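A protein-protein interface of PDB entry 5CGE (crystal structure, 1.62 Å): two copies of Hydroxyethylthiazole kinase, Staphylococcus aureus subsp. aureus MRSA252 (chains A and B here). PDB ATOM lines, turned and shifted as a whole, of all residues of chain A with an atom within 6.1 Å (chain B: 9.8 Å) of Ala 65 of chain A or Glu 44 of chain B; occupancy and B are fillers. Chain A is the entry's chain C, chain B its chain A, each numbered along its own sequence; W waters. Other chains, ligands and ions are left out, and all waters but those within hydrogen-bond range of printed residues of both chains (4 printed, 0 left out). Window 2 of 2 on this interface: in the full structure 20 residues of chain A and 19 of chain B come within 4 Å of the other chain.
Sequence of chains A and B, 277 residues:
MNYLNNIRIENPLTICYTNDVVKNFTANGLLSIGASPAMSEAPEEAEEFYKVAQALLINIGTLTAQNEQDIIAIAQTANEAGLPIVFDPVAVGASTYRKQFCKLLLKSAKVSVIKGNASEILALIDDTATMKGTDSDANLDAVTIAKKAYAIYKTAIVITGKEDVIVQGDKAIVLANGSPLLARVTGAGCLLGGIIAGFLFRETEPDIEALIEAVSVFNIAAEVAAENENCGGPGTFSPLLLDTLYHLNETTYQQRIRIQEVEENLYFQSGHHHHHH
OG of Ser 40 of chain B is in hydrogen-bond range of OE2 of Glu 45 of chain B (2.7 Å). The backbone NH (N) of Thr 64 of chain A is in hydrogen-bond range of the side-chain amide oxygen (OD1) of Asn 67 of chain A. The backbone NH (N) of Ala 65 of chain A sits at hydrogen-bond distance from the side-chain hydroxyl (OH) of Tyr 97 of chain A (3.3 Å). The side-chain carboxylate of Glu 68 of chain A lies within hydrogen-bond range of the side-chain hydroxyl of Tyr 97 of chain A (2.6 Å).
Thr 64 of chain A touches just one residue of chain B: Ala 42 (3.96 Å). No residue of chain B comes within 4 Å of Gln 66 of chain A. Of the printed residues of chain B, Ser 95 of chain A touches Glu 45, Glu 48 and Phe 49. Printed residues of chain B within 4 Å of Thr 96 of chain A: Glu 48 (2.9 Å). Tyr 17 of chain B touches none of the printed residues of chain A. Of the printed residues of chain A, Ala 42 of chain B touches Leu 63, Thr 64 and Tyr 97. Of chain A, only Ala 65 (3.9 Å) and Tyr 97 (3.6 Å) come within 4 Å of Glu 44 of chain B. Of the printed residues of chain A, Glu 45 of chain B touches Ser 95 and Tyr 97. Of the printed residues of chain A, Phe 49 of chain B touches Ser 95. Ile 74 of chain B touches none of the printed residues of chain A. The nearest residue of chain B that does not touch Ala 65 of chain A is Ala 42 of chain B (5.3 Å). The nearest printed residue of chain A that does not touch Phe 49 of chain B is Thr 96 of chain A (7.0 Å).
Water W4 lies within hydrogen-bond range of OE2 of Glu 48 of chain B, O of Glu 44 of chain B, N of Tyr 97 of chain A and OG1 of Thr 96 of chain A. Water W3 bridges OE2 of Glu 68 of chain A (2.6 Å) and OE2 of Glu 44 of chain B (2.8 Å). Water W2 lies within hydrogen-bond range of O of Leu 63 of chain A (2.7 Å), OE2 of Glu 45 of chain B (2.9 Å), N of Glu 41 of chain B (3.3 Å) and N of Ala 42 of chain B (3.3 Å). Water W1 lies within hydrogen-bond range of OE1 of Glu 44 of chain B (2.8 Å) and N of Ala 65 of chain A (2.9 Å).
Of the 10 printed residues of chain A, 6 touch a printed residue of chain B. Along chain A the printed residues that touch a printed residue of chain B span positions 63 to 97.
The side-chain carboxylate of Glu 45 of chain B sits at hydrogen-bond distance from the side-chain hydroxyl of Ser 95 of chain A (2.8 Å). The side-chain carboxylate (OE2) of Glu 48 of chain B sits at hydrogen-bond distance from the backbone NH (N) of Thr 96 of chain A (2.9 Å).
Among the printed residues, merely in contact across the chains: Ser 95 of chain A with Glu 48 of chain B, Leu 63 of chain A with Ala 42 of chain B, Tyr 97 of chain A with Glu 44 of chain B, Tyr 97 of chain A with Ala 42 of chain B, Tyr 97 of chain A with Glu 45 of chain B, Ser 95 of chain A with Phe 49 of chain B, Ala 65 of chain A with Glu 44 of chain B and Thr 64 of chain A with Ala 42 of chain B.
Position printed for both chains: 66. Of the 10 pairs that touch across the chains among the printed residues, none has its exchanged pair printed and touching as well.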
ATOM      1  N   LEU A  63     -16.359 -19.081  18.374  1.00  0.00           N
ATOM      2  CA  LEU A  63     -16.529 -17.959  19.315  1.00  0.00           C
ATOM      3  C   LEU A  63     -16.412 -18.457  20.745  1.00  0.00           C
ATOM      4  O   LEU A  63     -17.110 -19.422  21.190  1.00  0.00           O
ATOM      5  CB  LEU A  63     -17.921 -17.345  19.117  1.00  0.00           C
ATOM      6  CG  LEU A  63     -18.236 -16.126  19.928  1.00  0.00           C
ATOM      7  CD1 LEU A  63     -17.407 -14.994  19.412  1.00  0.00           C
ATOM      8  CD2 LEU A  63     -19.700 -15.827  19.809  1.00  0.00           C
ATOM      9  N   THR A  64     -15.617 -17.732  21.535  1.00  0.00           N
ATOM     10  CA  THR A  64     -15.517 -17.971  22.978  1.00  0.00           C
ATOM     11  C   THR A  64     -15.349 -16.605  23.663  1.00  0.00           C
ATOM     12  O   THR A  64     -15.133 -15.589  23.012  1.00  0.00           O
ATOM     13  CB  THR A  64     -14.316 -18.844  23.391  1.00  0.00           C
ATOM     14  OG1 THR A  64     -13.060 -18.249  23.006  1.00  0.00           O
ATOM     15  CG2 THR A  64     -14.387 -20.219  22.809  1.00  0.00           C
ATOM     16  N   ALA A  65     -15.368 -16.649  24.982  1.00  0.00           N
ATOM     17  CA  ALA A  65     -15.257 -15.398  25.786  1.00  0.00           C
ATOM     18  C   ALA A  65     -13.965 -14.665  25.439  1.00  0.00           C
ATOM     19  O   ALA A  65     -13.971 -13.422  25.390  1.00  0.00           O
ATOM     20  CB  ALA A  65     -15.325 -15.720  27.282  1.00  0.00           C
ATOM     21  N   GLN A  66     -12.920 -15.394  25.147  1.00  0.00           N
ATOM     22  CA  GLN A  66     -11.618 -14.797  24.719  1.00  0.00           C
ATOM     23  C   GLN A  66     -11.764 -13.844  23.504  1.00  0.00           C
ATOM     24  O   GLN A  66     -11.037 -12.846  23.421  1.00  0.00           O
ATOM     25  CB  GLN A  66     -10.630 -15.934  24.365  1.00  0.00           C
ATOM     26  N   ASN A  67     -12.686 -14.143  22.589  1.00  0.00           N
ATOM     27  CA  ASN A  67     -12.823 -13.435  21.345  1.00  0.00           C
ATOM     28  C   ASN A  67     -13.827 -12.281  21.417  1.00  0.00           C
ATOM     29  O   ASN A  67     -13.789 -11.354  20.604  1.00  0.00           O
ATOM     30  CB  ASN A  67     -13.372 -14.386  20.239  1.00  0.00           C
ATOM     31  CG  ASN A  67     -12.547 -15.601  20.008  1.00  0.00           C
ATOM     32  OD1 ASN A  67     -13.080 -16.700  20.022  1.00  0.00           O
ATOM     33  ND2 ASN A  67     -11.253 -15.448  19.779  1.00  0.00           N
ATOM     34  N   GLU A  68     -14.821 -12.374  22.271  1.00  0.00           N
ATOM     35  CA  GLU A  68     -15.979 -11.481  22.162  1.00  0.00           C
ATOM     36  C   GLU A  68     -15.653 -10.020  22.159  1.00  0.00           C
ATOM     37  O   GLU A  68     -16.063  -9.301  21.224  1.00  0.00           O
ATOM     38  CB  GLU A  68     -16.992 -11.739  23.253  1.00  0.00           C
ATOM     39  CG  GLU A  68     -17.671 -13.069  23.192  1.00  0.00           C
ATOM     40  CD  GLU A  68     -18.555 -13.331  24.423  1.00  0.00           C
ATOM     41  OE1 GLU A  68     -19.320 -12.407  24.814  1.00  0.00           O
ATOM     42  OE2 GLU A  68     -18.396 -14.389  25.066  1.00  0.00           O
ATOM     43  N   GLN A  69     -14.971  -9.534  23.192  1.00  0.00           N
ATOM     44  CA  GLN A  69     -14.694  -8.101  23.294  1.00  0.00           C
ATOM     45  C   GLN A  69     -13.700  -7.687  22.177  1.00  0.00           C
ATOM     46  O   GLN A  69     -13.820  -6.616  21.596  1.00  0.00           O
ATOM     47  CB  GLN A  69     -14.074  -7.706  24.662  1.00  0.00           C
ATOM     48  CG  GLN A  69     -14.855  -8.028  25.949  1.00  0.00           C
ATOM     49  CD  GLN A  69     -16.342  -8.036  25.767  1.00  0.00           C
ATOM     50  OE1 GLN A  69     -17.018  -9.061  26.001  1.00  0.00           O
ATOM     51  NE2 GLN A  69     -16.871  -6.905  25.414  1.00  0.00           N
ATOM     52  N   SER A  95     -27.262 -21.408  18.963  1.00  0.00           N
ATOM     53  CA  SER A  95     -27.220 -21.024  20.344  1.00  0.00           C
ATOM     54  C   SER A  95     -27.625 -19.605  20.590  1.00  0.00           C
ATOM     55  O   SER A  95     -27.319 -18.729  19.774  1.00  0.00           O
ATOM     56  CB  SER A  95     -25.851 -21.340  21.013  1.00  0.00           C
ATOM     57  OG  SER A  95     -24.830 -20.421  20.549  1.00  0.00           O
ATOM     58  N   THR A  96     -28.243 -19.356  21.737  1.00  0.00           N
ATOM     59  CA  THR A  96     -28.503 -18.016  22.173  1.00  0.00           C
ATOM     60  C   THR A  96     -27.205 -17.227  22.413  1.00  0.00           C
ATOM     61  O   THR A  96     -27.157 -16.018  22.133  1.00  0.00           O
ATOM     62  CB  THR A  96     -29.424 -17.962  23.412  1.00  0.00           C
ATOM     63  OG1 THR A  96     -28.754 -18.534  24.522  1.00  0.00           O
ATOM     64  CG2 THR A  96     -30.663 -18.760  23.136  1.00  0.00           C
ATOM     65  N   TYR A  97     -26.135 -17.916  22.826  1.00  0.00           N
ATOM     66  CA  TYR A  97     -24.840 -17.271  22.981  1.00  0.00           C
ATOM     67  C   TYR A  97     -24.419 -16.604  21.653  1.00  0.00           C
ATOM     68  O   TYR A  97     -24.008 -15.461  21.618  1.00  0.00           O
ATOM     69  CB  TYR A  97     -23.830 -18.314  23.422  1.00  0.00           C
ATOM     70  CG  TYR A  97     -22.410 -17.842  23.500  1.00  0.00           C
ATOM     71  CD1 TYR A  97     -22.046 -16.840  24.358  1.00  0.00           C
ATOM     72  CD2 TYR A  97     -21.443 -18.472  22.725  1.00  0.00           C
ATOM     73  CE1 TYR A  97     -20.721 -16.438  24.454  1.00  0.00           C
ATOM     74  CE2 TYR A  97     -20.114 -18.068  22.790  1.00  0.00           C
ATOM     75  CZ  TYR A  97     -19.763 -17.079  23.673  1.00  0.00           C
ATOM     76  OH  TYR A  97     -18.454 -16.644  23.690  1.00  0.00           O
ATOM     77  N   TYR B  17     -13.987 -30.869  21.532  1.00  0.00           N
ATOM     78  CA  TYR B  17     -13.096 -29.965  22.287  1.00  0.00           C
ATOM     79  C   TYR B  17     -11.710 -30.622  22.169  1.00  0.00           C
ATOM     80  O   TYR B  17     -11.391 -31.501  22.979  1.00  0.00           O
ATOM     81  CB  TYR B  17     -13.544 -29.842  23.746  1.00  0.00           C
ATOM     82  CG  TYR B  17     -12.955 -28.636  24.485  1.00  0.00           C
ATOM     83  CD1 TYR B  17     -11.608 -28.509  24.679  1.00  0.00           C
ATOM     84  CD2 TYR B  17     -13.763 -27.622  24.938  1.00  0.00           C
ATOM     85  CE1 TYR B  17     -11.050 -27.387  25.278  1.00  0.00           C
ATOM     86  CE2 TYR B  17     -13.242 -26.513  25.595  1.00  0.00           C
ATOM     87  CZ  TYR B  17     -11.876 -26.388  25.731  1.00  0.00           C
ATOM     88  OH  TYR B  17     -11.340 -25.246  26.342  1.00  0.00           O
ATOM     89  N   SER B  40     -17.040 -26.676  19.249  1.00  0.00           N
ATOM     90  CA  SER B  40     -17.554 -25.664  20.154  1.00  0.00           C
ATOM     91  C   SER B  40     -16.762 -25.803  21.474  1.00  0.00           C
ATOM     92  O   SER B  40     -16.698 -26.873  22.063  1.00  0.00           O
ATOM     93  CB  SER B  40     -19.017 -25.912  20.378  1.00  0.00           C
ATOM     94  OG  SER B  40     -19.548 -25.037  21.375  1.00  0.00           O
ATOM     95  N   GLU B  41     -16.189 -24.689  21.958  1.00  0.00           N
ATOM     96  CA  GLU B  41     -15.383 -24.676  23.163  1.00  0.00           C
ATOM     97  C   GLU B  41     -15.990 -23.733  24.212  1.00  0.00           C
ATOM     98  O   GLU B  41     -15.482 -23.659  25.304  1.00  0.00           O
ATOM     99  CB  GLU B  41     -13.968 -24.220  22.848  1.00  0.00           C
ATOM    100  CG  GLU B  41     -13.249 -25.272  22.007  1.00  0.00           C
ATOM    101  CD  GLU B  41     -11.769 -25.010  21.868  1.00  0.00           C
ATOM    102  OE1 GLU B  41     -11.236 -23.931  22.315  1.00  0.00           O
ATOM    103  OE2 GLU B  41     -11.111 -25.896  21.297  1.00  0.00           O
ATOM    104  N   ALA B  42     -17.013 -22.994  23.839  1.00  0.00           N
ATOM    105  CA  ALA B  42     -17.592 -22.021  24.797  1.00  0.00           C
ATOM    106  C   ALA B  42     -18.533 -22.721  25.771  1.00  0.00           C
ATOM    107  O   ALA B  42     -19.586 -23.246  25.361  1.00  0.00           O
ATOM    108  CB  ALA B  42     -18.319 -20.947  24.067  1.00  0.00           C
ATOM    109  N   PRO B  43     -18.229 -22.673  27.066  1.00  0.00           N
ATOM    110  CA  PRO B  43     -19.198 -23.267  28.027  1.00  0.00           C
ATOM    111  C   PRO B  43     -20.583 -22.646  27.962  1.00  0.00           C
ATOM    112  O   PRO B  43     -21.564 -23.313  28.292  1.00  0.00           O
ATOM    113  CB  PRO B  43     -18.551 -22.990  29.397  1.00  0.00           C
ATOM    114  CG  PRO B  43     -17.141 -22.864  29.082  1.00  0.00           C
ATOM    115  CD  PRO B  43     -17.014 -22.225  27.726  1.00  0.00           C
ATOM    116  N   GLU B  44     -20.652 -21.394  27.530  1.00  0.00           N
ATOM    117  CA  GLU B  44     -21.930 -20.636  27.431  1.00  0.00           C
ATOM    118  C   GLU B  44     -22.907 -21.232  26.467  1.00  0.00           C
ATOM    119  O   GLU B  44     -24.105 -20.929  26.528  1.00  0.00           O
ATOM    120  CB  GLU B  44     -21.628 -19.191  27.012  1.00  0.00           C
ATOM    121  CG  GLU B  44     -20.806 -18.410  28.025  1.00  0.00           C
ATOM    122  CD  GLU B  44     -19.291 -18.447  27.835  1.00  0.00           C
ATOM    123  OE1 GLU B  44     -18.739 -19.365  27.162  1.00  0.00           O
ATOM    124  OE2 GLU B  44     -18.612 -17.569  28.430  1.00  0.00           O
ATOM    125  N   GLU B  45     -22.443 -22.010  25.475  1.00  0.00           N
ATOM    126  CA  GLU B  45     -23.352 -22.638  24.549  1.00  0.00           C
ATOM    127  C   GLU B  45     -23.414 -24.174  24.696  1.00  0.00           C
ATOM    128  O   GLU B  45     -24.100 -24.849  23.925  1.00  0.00           O
ATOM    129  CB  GLU B  45     -23.036 -22.249  23.111  1.00  0.00           C
ATOM    130  CG  GLU B  45     -21.744 -22.791  22.548  1.00  0.00           C
ATOM    131  CD  GLU B  45     -21.432 -22.269  21.135  1.00  0.00           C
ATOM    132  OE1 GLU B  45     -22.232 -21.464  20.595  1.00  0.00           O
ATOM    133  OE2 GLU B  45     -20.405 -22.647  20.556  1.00  0.00           O
ATOM    134  N   ALA B  46     -22.750 -24.712  25.723  1.00  0.00           N
ATOM    135  CA  ALA B  46     -22.718 -26.202  25.863  1.00  0.00           C
ATOM    136  C   ALA B  46     -24.044 -26.808  26.170  1.00  0.00           C
ATOM    137  O   ALA B  46     -24.467 -27.809  25.564  1.00  0.00           O
ATOM    138  CB  ALA B  46     -21.707 -26.581  26.951  1.00  0.00           C
ATOM    139  N   GLU B  47     -24.820 -26.187  27.045  1.00  0.00           N
ATOM    140  CA  GLU B  47     -26.148 -26.760  27.355  1.00  0.00           C
ATOM    141  C   GLU B  47     -27.036 -26.866  26.081  1.00  0.00           C
ATOM    142  O   GLU B  47     -27.587 -27.946  25.777  1.00  0.00           O
ATOM    143  CB  GLU B  47     -26.810 -25.973  28.501  1.00  0.00           C
ATOM    144  CG  GLU B  47     -27.940 -26.700  29.186  1.00  0.00           C
ATOM    145  CD  GLU B  47     -28.606 -25.876  30.269  1.00  0.00           C
ATOM    146  OE1 GLU B  47     -27.946 -24.973  30.823  1.00  0.00           O
ATOM    147  OE2 GLU B  47     -29.813 -26.121  30.543  1.00  0.00           O
ATOM    148  N   GLU B  48     -27.097 -25.826  25.275  1.00  0.00           N
ATOM    149  CA  GLU B  48     -27.900 -25.881  24.043  1.00  0.00           C
ATOM    150  C   GLU B  48     -27.360 -26.841  22.996  1.00  0.00           C
ATOM    151  O   GLU B  48     -28.122 -27.594  22.398  1.00  0.00           O
ATOM    152  CB  GLU B  48     -28.026 -24.480  23.424  1.00  0.00           C
ATOM    153  CG  GLU B  48     -28.983 -23.571  24.140  1.00  0.00           C
ATOM    154  CD  GLU B  48     -29.112 -22.269  23.379  1.00  0.00           C
ATOM    155  OE1 GLU B  48     -29.794 -22.250  22.320  1.00  0.00           O
ATOM    156  OE2 GLU B  48     -28.490 -21.308  23.806  1.00  0.00           O
ATOM    157  N   PHE B  49     -26.047 -26.823  22.776  1.00  0.00           N
ATOM    158  CA  PHE B  49     -25.461 -27.726  21.807  1.00  0.00           C
ATOM    159  C   PHE B  49     -25.633 -29.182  22.258  1.00  0.00           C
ATOM    160  O   PHE B  49     -25.872 -30.040  21.429  1.00  0.00           O
ATOM    161  CB  PHE B  49     -23.927 -27.416  21.621  1.00  0.00           C
ATOM    162  CG  PHE B  49     -23.599 -26.460  20.499  1.00  0.00           C
ATOM    163  CD1 PHE B  49     -24.105 -25.182  20.478  1.00  0.00           C
ATOM    164  CD2 PHE B  49     -22.856 -26.839  19.417  1.00  0.00           C
ATOM    165  CE1 PHE B  49     -23.867 -24.323  19.413  1.00  0.00           C
ATOM    166  CE2 PHE B  49     -22.559 -25.960  18.362  1.00  0.00           C
ATOM    167  CZ  PHE B  49     -23.041 -24.661  18.399  1.00  0.00           C
ATOM    168  N   TYR B  50     -25.425 -29.459  23.528  1.00  0.00           N
ATOM    169  CA  TYR B  50     -25.331 -30.842  23.994  1.00  0.00           C
ATOM    170  C   TYR B  50     -26.680 -31.530  23.987  1.00  0.00           C
ATOM    171  O   TYR B  50     -26.738 -32.738  23.763  1.00  0.00           O
ATOM    172  CB  TYR B  50     -24.694 -30.916  25.384  1.00  0.00           C
ATOM    173  CG  TYR B  50     -23.242 -30.568  25.469  1.00  0.00           C
ATOM    174  CD1 TYR B  50     -22.528 -30.104  24.373  1.00  0.00           C
ATOM    175  CD2 TYR B  50     -22.546 -30.687  26.671  1.00  0.00           C
ATOM    176  CE1 TYR B  50     -21.204 -29.762  24.497  1.00  0.00           C
ATOM    177  CE2 TYR B  50     -21.212 -30.407  26.767  1.00  0.00           C
ATOM    178  CZ  TYR B  50     -20.537 -29.898  25.684  1.00  0.00           C
ATOM    179  OH  TYR B  50     -19.203 -29.584  25.730  1.00  0.00           O
ATOM    180  N   GLN B  66      -6.028 -21.589  29.993  1.00  0.00           N
ATOM    181  CA  GLN B  66      -7.273 -21.177  29.271  1.00  0.00           C
ATOM    182  C   GLN B  66      -8.345 -22.270  29.218  1.00  0.00           C
ATOM    183  O   GLN B  66      -9.543 -21.971  29.248  1.00  0.00           O
ATOM    184  CB  GLN B  66      -6.885 -20.770  27.824  1.00  0.00           C
ATOM    185  CG  GLN B  66      -8.005 -20.465  26.844  1.00  0.00           C
ATOM    186  N   ASP B  70     -12.742 -24.623  31.787  1.00  0.00           N
ATOM    187  CA  ASP B  70     -13.781 -24.783  30.745  1.00  0.00           C
ATOM    188  C   ASP B  70     -14.009 -26.247  30.443  1.00  0.00           C
ATOM    189  O   ASP B  70     -15.179 -26.691  30.327  1.00  0.00           O
ATOM    190  CB  ASP B  70     -13.423 -24.048  29.449  1.00  0.00           C
ATOM    191  CG  ASP B  70     -13.569 -22.507  29.561  1.00  0.00           C
ATOM    192  OD1 ASP B  70     -14.044 -21.996  30.618  1.00  0.00           O
ATOM    193  OD2 ASP B  70     -13.201 -21.843  28.595  1.00  0.00           O
ATOM    194  N   ALA B  73     -15.970 -27.730  33.276  1.00  0.00           N
ATOM    195  CA  ALA B  73     -17.374 -27.266  33.235  1.00  0.00           C
ATOM    196  C   ALA B  73     -18.141 -27.981  32.148  1.00  0.00           C
ATOM    197  O   ALA B  73     -19.296 -28.438  32.380  1.00  0.00           O
ATOM    198  CB  ALA B  73     -17.434 -25.747  33.029  1.00  0.00           C
ATOM    199  N   ILE B  74     -17.573 -28.087  30.936  1.00  0.00           N
ATOM    200  CA  ILE B  74     -18.330 -28.708  29.850  1.00  0.00           C
ATOM    201  C   ILE B  74     -18.506 -30.205  30.078  1.00  0.00           C
ATOM    202  O   ILE B  74     -19.500 -30.786  29.667  1.00  0.00           O
ATOM    203  CB  ILE B  74     -17.791 -28.430  28.435  1.00  0.00           C
ATOM    204  CG1 ILE B  74     -16.445 -29.085  28.253  1.00  0.00           C
ATOM    205  CG2 ILE B  74     -17.827 -26.939  28.142  1.00  0.00           C
ATOM    206  CD1 ILE B  74     -15.976 -29.172  26.859  1.00  0.00           C
ATOM    207  N   THR B  77     -21.475 -30.373  32.170  1.00  0.00           N
ATOM    208  CA  THR B  77     -22.653 -30.118  31.333  1.00  0.00           C
ATOM    209  C   THR B  77     -23.007 -31.340  30.492  1.00  0.00           C
ATOM    210  O   THR B  77     -24.168 -31.722  30.394  1.00  0.00           O
ATOM    211  CB  THR B  77     -22.443 -28.897  30.425  1.00  0.00           C
ATOM    212  OG1 THR B  77     -22.115 -27.798  31.230  1.00  0.00           O
ATOM    213  CG2 THR B  77     -23.692 -28.612  29.602  1.00  0.00           C
HETATM  214  O   HOH W   1     -16.182 -19.165  26.116  1.00  0.00           O
HETATM  215  O   HOH W   2     -17.587 -21.986  20.706  1.00  0.00           O
HETATM  216  O   HOH W   3     -19.001 -14.953  27.523  1.00  0.00           O
HETATM  217  O   HOH W   4     -26.261 -20.444  24.562  1.00  0.00           O
